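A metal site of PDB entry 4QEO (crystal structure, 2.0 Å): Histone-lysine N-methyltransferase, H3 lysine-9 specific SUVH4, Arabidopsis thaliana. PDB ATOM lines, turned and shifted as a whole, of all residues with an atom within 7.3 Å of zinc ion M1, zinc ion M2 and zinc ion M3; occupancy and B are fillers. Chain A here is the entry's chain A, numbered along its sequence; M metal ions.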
ATOM      1  N   THR A 290      25.458 -11.589 -12.203  1.00  0.00           N
ATOM      2  CA  THR A 290      25.427 -11.499 -10.746  1.00  0.00           C
ATOM      3  C   THR A 290      24.359 -12.420 -10.166  1.00  0.00           C
ATOM      4  O   THR A 290      24.586 -13.097  -9.166  1.00  0.00           O
ATOM      5  CB  THR A 290      25.158 -10.057 -10.283  1.00  0.00           C
ATOM      6  OG1 THR A 290      26.273  -9.239 -10.635  1.00  0.00           O
ATOM      7  CG2 THR A 290      24.959 -10.019  -8.770  1.00  0.00           C
ATOM      8  N   GLY A 291      23.192 -12.428 -10.780  1.00  0.00           N
ATOM      9  CA  GLY A 291      22.122 -13.300 -10.348  1.00  0.00           C
ATOM     10  C   GLY A 291      21.271 -12.718  -9.238  1.00  0.00           C
ATOM     11  O   GLY A 291      21.524 -11.611  -8.766  1.00  0.00           O
ATOM     12  N   CYS A 292      20.253 -13.480  -8.829  1.00  0.00           N
ATOM     13  CA  CYS A 292      19.288 -13.033  -7.836  1.00  0.00           C
ATOM     14  C   CYS A 292      19.561 -13.638  -6.465  1.00  0.00           C
ATOM     15  O   CYS A 292      20.351 -14.584  -6.346  1.00  0.00           O
ATOM     16  CB  CYS A 292      17.868 -13.414  -8.307  1.00  0.00           C
ATOM     17  SG  CYS A 292      17.524 -15.215  -8.358  1.00  0.00           S
ATOM     18  N   ASN A 293      18.898 -13.128  -5.435  1.00  0.00           N
ATOM     19  CA  ASN A 293      19.174 -13.573  -4.071  1.00  0.00           C
ATOM     20  C   ASN A 293      18.054 -14.405  -3.451  1.00  0.00           C
ATOM     21  O   ASN A 293      18.021 -14.603  -2.240  1.00  0.00           O
ATOM     22  CB  ASN A 293      19.515 -12.397  -3.152  1.00  0.00           C
ATOM     23  CG  ASN A 293      18.331 -11.477  -2.927  1.00  0.00           C
ATOM     24  OD1 ASN A 293      17.398 -11.810  -2.200  1.00  0.00           O
ATOM     25  ND2 ASN A 293      18.375 -10.309  -3.548  1.00  0.00           N
ATOM     26  N   CYS A 294      17.136 -14.892  -4.282  1.00  0.00           N
ATOM     27  CA  CYS A 294      16.000 -15.667  -3.786  1.00  0.00           C
ATOM     28  C   CYS A 294      16.459 -16.995  -3.182  1.00  0.00           C
ATOM     29  O   CYS A 294      17.500 -17.525  -3.560  1.00  0.00           O
ATOM     30  CB  CYS A 294      15.003 -15.912  -4.929  1.00  0.00           C
ATOM     31  SG  CYS A 294      14.536 -14.422  -5.850  1.00  0.00           S
ATOM     32  N   ARG A 295      15.689 -17.524  -2.250  1.00  0.00           N
ATOM     33  CA  ARG A 295      15.980 -18.832  -1.685  1.00  0.00           C
ATOM     34  C   ARG A 295      14.999 -19.885  -2.212  1.00  0.00           C
ATOM     35  O   ARG A 295      13.797 -19.639  -2.290  1.00  0.00           O
ATOM     36  CB  ARG A 295      15.878 -18.784  -0.163  1.00  0.00           C
ATOM     37  CG  ARG A 295      16.970 -17.960   0.523  1.00  0.00           C
ATOM     38  CD  ARG A 295      16.538 -17.574   1.925  1.00  0.00           C
ATOM     39  NE  ARG A 295      15.816 -18.660   2.586  1.00  0.00           N
ATOM     40  CZ  ARG A 295      16.178 -19.223   3.734  1.00  0.00           C
ATOM     41  NH1 ARG A 295      17.260 -18.793   4.369  1.00  0.00           N
ATOM     42  NH2 ARG A 295      15.456 -20.201   4.255  1.00  0.00           N
ATOM     43  N   GLY A 296      15.521 -21.055  -2.583  1.00  0.00           N
ATOM     44  CA  GLY A 296      14.681 -22.156  -3.009  1.00  0.00           C
ATOM     45  C   GLY A 296      14.178 -22.040  -4.433  1.00  0.00           C
ATOM     46  O   GLY A 296      14.717 -22.687  -5.331  1.00  0.00           O
ATOM     47  N   SER A 297      13.143 -21.235  -4.639  1.00  0.00           N
ATOM     48  CA  SER A 297      12.614 -20.968  -5.977  1.00  0.00           C
ATOM     49  C   SER A 297      12.208 -19.513  -6.135  1.00  0.00           C
ATOM     50  O   SER A 297      11.820 -18.858  -5.182  1.00  0.00           O
ATOM     51  CB  SER A 297      11.423 -21.877  -6.276  1.00  0.00           C
ATOM     52  OG  SER A 297      11.835 -23.223  -6.424  1.00  0.00           O
ATOM     53  N   CYS A 298      12.312 -18.995  -7.357  1.00  0.00           N
ATOM     54  CA  CYS A 298      11.997 -17.597  -7.624  1.00  0.00           C
ATOM     55  C   CYS A 298      10.525 -17.434  -8.003  1.00  0.00           C
ATOM     56  O   CYS A 298      10.076 -17.964  -9.028  1.00  0.00           O
ATOM     57  CB  CYS A 298      12.895 -17.048  -8.725  1.00  0.00           C
ATOM     58  SG  CYS A 298      14.669 -17.286  -8.354  1.00  0.00           S
ATOM     59  N   THR A 299       9.788 -16.712  -7.153  1.00  0.00           N
ATOM     60  CA  THR A 299       8.337 -16.606  -7.273  1.00  0.00           C
ATOM     61  C   THR A 299       7.845 -15.160  -7.325  1.00  0.00           C
ATOM     62  O   THR A 299       6.878 -14.841  -8.017  1.00  0.00           O
ATOM     63  CB  THR A 299       7.645 -17.315  -6.096  1.00  0.00           C
ATOM     64  OG1 THR A 299       8.150 -16.782  -4.856  1.00  0.00           O
ATOM     65  CG2 THR A 299       7.913 -18.806  -6.146  1.00  0.00           C
ATOM     66  N   ASP A 300       8.527 -14.278  -6.596  1.00  0.00           N
ATOM     67  CA  ASP A 300       8.103 -12.889  -6.553  1.00  0.00           C
ATOM     68  C   ASP A 300       8.915 -12.011  -7.486  1.00  0.00           C
ATOM     69  O   ASP A 300      10.139 -11.900  -7.339  1.00  0.00           O
ATOM     70  CB  ASP A 300       8.167 -12.355  -5.127  1.00  0.00           C
ATOM     71  CG  ASP A 300       8.139 -10.849  -5.053  1.00  0.00           C
ATOM     72  OD1 ASP A 300       7.475 -10.198  -5.893  1.00  0.00           O
ATOM     73  OD2 ASP A 300       8.772 -10.298  -4.126  1.00  0.00           O
ATOM     74  N   LYS A 303      11.135  -9.000  -5.621  1.00  0.00           N
ATOM     75  CA  LYS A 303      12.458  -9.342  -5.089  1.00  0.00           C
ATOM     76  C   LYS A 303      13.453  -9.772  -6.165  1.00  0.00           C
ATOM     77  O   LYS A 303      14.559  -9.216  -6.254  1.00  0.00           O
ATOM     78  CB  LYS A 303      12.332 -10.435  -4.019  1.00  0.00           C
ATOM     79  CG  LYS A 303      11.648  -9.960  -2.739  1.00  0.00           C
ATOM     80  CD  LYS A 303      11.218 -11.127  -1.862  1.00  0.00           C
ATOM     81  CE  LYS A 303      10.124 -10.701  -0.882  1.00  0.00           C
ATOM     82  NZ  LYS A 303      10.608  -9.809   0.206  1.00  0.00           N
ATOM     83  N   CYS A 304      13.057 -10.739  -6.983  1.00  0.00           N
ATOM     84  CA  CYS A 304      13.948 -11.384  -7.942  1.00  0.00           C
ATOM     85  C   CYS A 304      14.473 -10.489  -9.070  1.00  0.00           C
ATOM     86  O   CYS A 304      13.708 -10.047  -9.926  1.00  0.00           O
ATOM     87  CB  CYS A 304      13.272 -12.601  -8.571  1.00  0.00           C
ATOM     88  SG  CYS A 304      14.417 -13.485  -9.656  1.00  0.00           S
ATOM     89  N   ALA A 305      15.782 -10.282  -9.079  1.00  0.00           N
ATOM     90  CA  ALA A 305      16.456  -9.487 -10.110  1.00  0.00           C
ATOM     91  C   ALA A 305      16.363 -10.112 -11.504  1.00  0.00           C
ATOM     92  O   ALA A 305      16.428  -9.414 -12.523  1.00  0.00           O
ATOM     93  CB  ALA A 305      17.916  -9.299  -9.741  1.00  0.00           C
ATOM     94  N   CYS A 306      16.252 -11.429 -11.572  1.00  0.00           N
ATOM     95  CA  CYS A 306      16.228 -12.080 -12.867  1.00  0.00           C
ATOM     96  C   CYS A 306      14.895 -11.763 -13.568  1.00  0.00           C
ATOM     97  O   CYS A 306      14.844 -11.454 -14.778  1.00  0.00           O
ATOM     98  CB  CYS A 306      16.522 -13.590 -12.727  1.00  0.00           C
ATOM     99  SG  CYS A 306      18.101 -13.990 -11.790  1.00  0.00           S
ATOM    100  N   ALA A 307      13.822 -11.753 -12.784  1.00  0.00           N
ATOM    101  CA  ALA A 307      12.521 -11.307 -13.283  1.00  0.00           C
ATOM    102  C   ALA A 307      12.627  -9.883 -13.818  1.00  0.00           C
ATOM    103  O   ALA A 307      12.131  -9.583 -14.914  1.00  0.00           O
ATOM    104  CB  ALA A 307      11.487 -11.369 -12.176  1.00  0.00           C
ATOM    105  N   PHE A 314       8.110 -13.109 -14.856  1.00  0.00           N
ATOM    106  CA  PHE A 314       8.678 -14.403 -15.212  1.00  0.00           C
ATOM    107  C   PHE A 314       8.199 -14.875 -16.587  1.00  0.00           C
ATOM    108  O   PHE A 314       6.996 -14.858 -16.866  1.00  0.00           O
ATOM    109  CB  PHE A 314       8.374 -15.447 -14.146  1.00  0.00           C
ATOM    110  CG  PHE A 314       9.028 -15.150 -12.831  1.00  0.00           C
ATOM    111  CD1 PHE A 314      10.369 -15.434 -12.632  1.00  0.00           C
ATOM    112  CD2 PHE A 314       8.307 -14.556 -11.802  1.00  0.00           C
ATOM    113  CE1 PHE A 314      10.978 -15.137 -11.417  1.00  0.00           C
ATOM    114  CE2 PHE A 314       8.909 -14.266 -10.590  1.00  0.00           C
ATOM    115  CZ  PHE A 314      10.252 -14.565 -10.397  1.00  0.00           C
ATOM    116  N   PHE A 332      15.896 -14.359 -19.789  1.00  0.00           N
ATOM    117  CA  PHE A 332      16.924 -14.262 -18.754  1.00  0.00           C
ATOM    118  C   PHE A 332      16.648 -15.261 -17.647  1.00  0.00           C
ATOM    119  O   PHE A 332      15.791 -15.040 -16.789  1.00  0.00           O
ATOM    120  CB  PHE A 332      16.988 -12.859 -18.170  1.00  0.00           C
ATOM    121  CG  PHE A 332      17.537 -11.820 -19.106  1.00  0.00           C
ATOM    122  CD1 PHE A 332      18.901 -11.618 -19.213  1.00  0.00           C
ATOM    123  CD2 PHE A 332      16.688 -11.024 -19.860  1.00  0.00           C
ATOM    124  CE1 PHE A 332      19.422 -10.647 -20.062  1.00  0.00           C
ATOM    125  CE2 PHE A 332      17.192 -10.050 -20.709  1.00  0.00           C
ATOM    126  CZ  PHE A 332      18.557  -9.868 -20.809  1.00  0.00           C
ATOM    127  N   GLU A 333      17.384 -16.367 -17.674  1.00  0.00           N
ATOM    128  CA  GLU A 333      17.220 -17.400 -16.682  1.00  0.00           C
ATOM    129  C   GLU A 333      18.136 -17.190 -15.495  1.00  0.00           C
ATOM    130  O   GLU A 333      19.180 -16.529 -15.592  1.00  0.00           O
ATOM    131  CB  GLU A 333      17.491 -18.779 -17.295  1.00  0.00           C
ATOM    132  CG  GLU A 333      16.315 -19.353 -18.080  1.00  0.00           C
ATOM    133  CD  GLU A 333      16.547 -20.771 -18.573  1.00  0.00           C
ATOM    134  OE1 GLU A 333      17.644 -21.334 -18.325  1.00  0.00           O
ATOM    135  OE2 GLU A 333      15.641 -21.323 -19.209  1.00  0.00           O
ATOM    136  N   CYS A 334      17.734 -17.767 -14.369  1.00  0.00           N
ATOM    137  CA  CYS A 334      18.597 -17.866 -13.211  1.00  0.00           C
ATOM    138  C   CYS A 334      19.857 -18.654 -13.572  1.00  0.00           C
ATOM    139  O   CYS A 334      19.828 -19.548 -14.437  1.00  0.00           O
ATOM    140  CB  CYS A 334      17.850 -18.497 -12.029  1.00  0.00           C
ATOM    141  SG  CYS A 334      16.506 -17.454 -11.332  1.00  0.00           S
ATOM    142  N   GLY A 335      20.964 -18.302 -12.936  1.00  0.00           N
ATOM    143  CA  GLY A 335      22.253 -18.861 -13.284  1.00  0.00           C
ATOM    144  C   GLY A 335      23.064 -19.369 -12.102  1.00  0.00           C
ATOM    145  O   GLY A 335      22.521 -19.560 -11.016  1.00  0.00           O
ATOM    146  N   HIS A 337      25.218 -18.119 -10.018  1.00  0.00           N
ATOM    147  CA  HIS A 337      25.277 -17.340  -8.786  1.00  0.00           C
ATOM    148  C   HIS A 337      23.930 -17.034  -8.136  1.00  0.00           C
ATOM    149  O   HIS A 337      23.892 -16.381  -7.086  1.00  0.00           O
ATOM    150  CB  HIS A 337      26.083 -16.036  -8.997  1.00  0.00           C
ATOM    151  CG  HIS A 337      27.536 -16.271  -9.214  1.00  0.00           C
ATOM    152  ND1 HIS A 337      28.155 -16.065 -10.427  1.00  0.00           N
ATOM    153  CD2 HIS A 337      28.501 -16.742  -8.383  1.00  0.00           C
ATOM    154  CE1 HIS A 337      29.433 -16.374 -10.332  1.00  0.00           C
ATOM    155  NE2 HIS A 337      29.663 -16.789  -9.101  1.00  0.00           N
ATOM    156  N   CYS A 338      22.825 -17.468  -8.735  1.00  0.00           N
ATOM    157  CA  CYS A 338      21.518 -17.242  -8.121  1.00  0.00           C
ATOM    158  C   CYS A 338      21.351 -18.108  -6.876  1.00  0.00           C
ATOM    159  O   CYS A 338      21.862 -19.229  -6.820  1.00  0.00           O
ATOM    160  CB  CYS A 338      20.364 -17.502  -9.103  1.00  0.00           C
ATOM    161  SG  CYS A 338      20.345 -16.344 -10.487  1.00  0.00           S
ATOM    162  N   GLY A 339      20.617 -17.592  -5.892  1.00  0.00           N
ATOM    163  CA  GLY A 339      20.447 -18.272  -4.629  1.00  0.00           C
ATOM    164  C   GLY A 339      19.482 -19.439  -4.714  1.00  0.00           C
ATOM    165  O   GLY A 339      19.419 -20.255  -3.793  1.00  0.00           O
ATOM    166  N   CYS A 340      18.738 -19.521  -5.807  1.00  0.00           N
ATOM    167  CA  CYS A 340      17.706 -20.532  -6.002  1.00  0.00           C
ATOM    168  C   CYS A 340      18.312 -21.868  -6.396  1.00  0.00           C
ATOM    169  O   CYS A 340      19.380 -21.926  -7.024  1.00  0.00           O
ATOM    170  CB  CYS A 340      16.741 -20.074  -7.096  1.00  0.00           C
ATOM    171  SG  CYS A 340      17.567 -19.772  -8.680  1.00  0.00           S
ATOM    172  N   GLY A 341      17.618 -22.936  -6.038  1.00  0.00           N
ATOM    173  CA  GLY A 341      18.016 -24.280  -6.413  1.00  0.00           C
ATOM    174  C   GLY A 341      17.538 -24.652  -7.802  1.00  0.00           C
ATOM    175  O   GLY A 341      16.865 -23.876  -8.466  1.00  0.00           O
ATOM    176  N   LYS A 343      15.330 -26.436  -9.017  1.00  0.00           N
ATOM    177  CA  LYS A 343      13.911 -26.587  -9.286  1.00  0.00           C
ATOM    178  C   LYS A 343      13.249 -25.277  -9.708  1.00  0.00           C
ATOM    179  O   LYS A 343      12.088 -25.264 -10.093  1.00  0.00           O
ATOM    180  CB  LYS A 343      13.192 -27.148  -8.047  1.00  0.00           C
ATOM    181  CG  LYS A 343      13.410 -28.642  -7.812  1.00  0.00           C
ATOM    182  CD  LYS A 343      12.606 -29.125  -6.599  1.00  0.00           C
ATOM    183  CE  LYS A 343      12.905 -30.587  -6.251  1.00  0.00           C
ATOM    184  NZ  LYS A 343      12.313 -30.975  -4.909  1.00  0.00           N
ATOM    185  N   CYS A 344      13.989 -24.173  -9.611  1.00  0.00           N
ATOM    186  CA  CYS A 344      13.444 -22.849  -9.939  1.00  0.00           C
ATOM    187  C   CYS A 344      12.823 -22.856 -11.317  1.00  0.00           C
ATOM    188  O   CYS A 344      13.402 -23.381 -12.273  1.00  0.00           O
ATOM    189  CB  CYS A 344      14.517 -21.757  -9.863  1.00  0.00           C
ATOM    190  SG  CYS A 344      13.890 -20.118 -10.332  1.00  0.00           S
ATOM    191  N   VAL A 345      11.634 -22.271 -11.447  1.00  0.00           N
ATOM    192  CA  VAL A 345      10.942 -22.294 -12.743  1.00  0.00           C
ATOM    193  C   VAL A 345      11.667 -21.396 -13.748  1.00  0.00           C
ATOM    194  O   VAL A 345      11.631 -21.623 -14.965  1.00  0.00           O
ATOM    195  CB  VAL A 345       9.446 -21.937 -12.587  1.00  0.00           C
ATOM    196  CG1 VAL A 345       8.702 -22.093 -13.913  1.00  0.00           C
ATOM    197  CG2 VAL A 345       8.817 -22.833 -11.547  1.00  0.00           C
ATOM    198  N   ASN A 346      12.391 -20.415 -13.214  1.00  0.00           N
ATOM    199  CA  ASN A 346      13.209 -19.578 -14.071  1.00  0.00           C
ATOM    200  C   ASN A 346      14.536 -20.234 -14.477  1.00  0.00           C
ATOM    201  O   ASN A 346      15.433 -19.584 -15.001  1.00  0.00           O
ATOM    202  CB  ASN A 346      13.426 -18.175 -13.488  1.00  0.00           C
ATOM    203  CG  ASN A 346      13.698 -17.141 -14.559  1.00  0.00           C
ATOM    204  OD1 ASN A 346      13.062 -17.133 -15.598  1.00  0.00           O
ATOM    205  ND2 ASN A 346      14.687 -16.290 -14.321  1.00  0.00           N
ATOM    206  N   ARG A 347      14.651 -21.537 -14.227  1.00  0.00           N
ATOM    207  CA  ARG A 347      15.687 -22.343 -14.832  1.00  0.00           C
ATOM    208  C   ARG A 347      15.084 -23.374 -15.797  1.00  0.00           C
ATOM    209  O   ARG A 347      15.708 -24.408 -16.059  1.00  0.00           O
ATOM    210  CB  ARG A 347      16.495 -23.077 -13.745  1.00  0.00           C
ATOM    211  CG  ARG A 347      17.179 -22.149 -12.725  1.00  0.00           C
ATOM    212  CD  ARG A 347      17.885 -22.976 -11.662  1.00  0.00           C
ATOM    213  NE  ARG A 347      18.629 -22.182 -10.676  1.00  0.00           N
ATOM    214  CZ  ARG A 347      19.892 -21.798 -10.824  1.00  0.00           C
ATOM    215  NH1 ARG A 347      20.554 -22.095 -11.940  1.00  0.00           N
ATOM    216  NH2 ARG A 347      20.507 -21.113  -9.862  1.00  0.00           N
HETATM  217 ZN    ZN M   1      15.206 -14.977  -8.086  1.00  0.00          ZN
HETATM  218 ZN    ZN M   2      18.051 -15.700 -10.521  1.00  0.00          ZN
HETATM  219 ZN    ZN M   3      15.672 -18.684  -9.671  1.00  0.00          ZN
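Zinc ion M1 is bound by SG of Cys 304 (2.3 Å), SG of Cys 292 (2.3 Å), SG of Cys 298 (2.4 Å) and SG of Cys 294 (2.4 Å).
Zinc ion M1 has four donor atoms within binding distance.
Within 4 Å of zinc ion M2: Cys 292, Cys 306, Cys 334 and Cys 338.
The nearest printed residue that does not touch zinc ion M2 is Cys 298 (4.3 Å).
Of the 31 residues printed, 4 come within 4 Å of zinc ion M1.
The nearest printed residue that does not touch zinc ion M1 is Cys 334 (4.3 Å).
N of Ala 307 lies close to SG of Cys 304, at 3.6 Å.
The backbone carbonyl oxygen (O) of Cys 292 lies within hydrogen-bond range of the backbone NH (N) of Gly 339 (3.1 Å).
SG of Cys 344 lies close to N of Asn 346 (3.3 Å).
The backbone carbonyl oxygen (O) of Cys 340 sits at hydrogen-bond distance from the guanidinium group (NH2) of Arg 347, at 3.2 Å.
N of Cys 340 lies within hydrogen-bond range of O of Cys 294, 3.3 Å away.
SG of Cys 338 lies close to N of Gly 335 (3.2 Å).
The backbone NH (N) of Cys 306 sits close to the side-chain sulfur (SG) of Cys 304, 3.4 Å away.
The backbone carbonyl oxygen of Asn 346 is in hydrogen-bond range of the backbone NH of Cys 334.
Zinc ion M3 is bound by SG of Cys 298 (2.2 Å), SG of Cys 334 (2.2 Å), SG of Cys 344 (2.4 Å) and SG of Cys 340 (2.4 Å).
Zinc ion M3 has four donor atoms within binding distance.
SG of Cys 306 is bound to zinc ion M2 (2.1 Å).
Zinc ion M2 is bound by the side-chain sulfur (SG) of Cys 292, 2.3 Å away.
Zinc ion M2 is bound by SG of Cys 338 (2.4 Å).
Zinc ion M2 is bound by the side-chain sulfur (SG) of Cys 334.
Zinc ion M2 has four donor atoms within binding distance.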
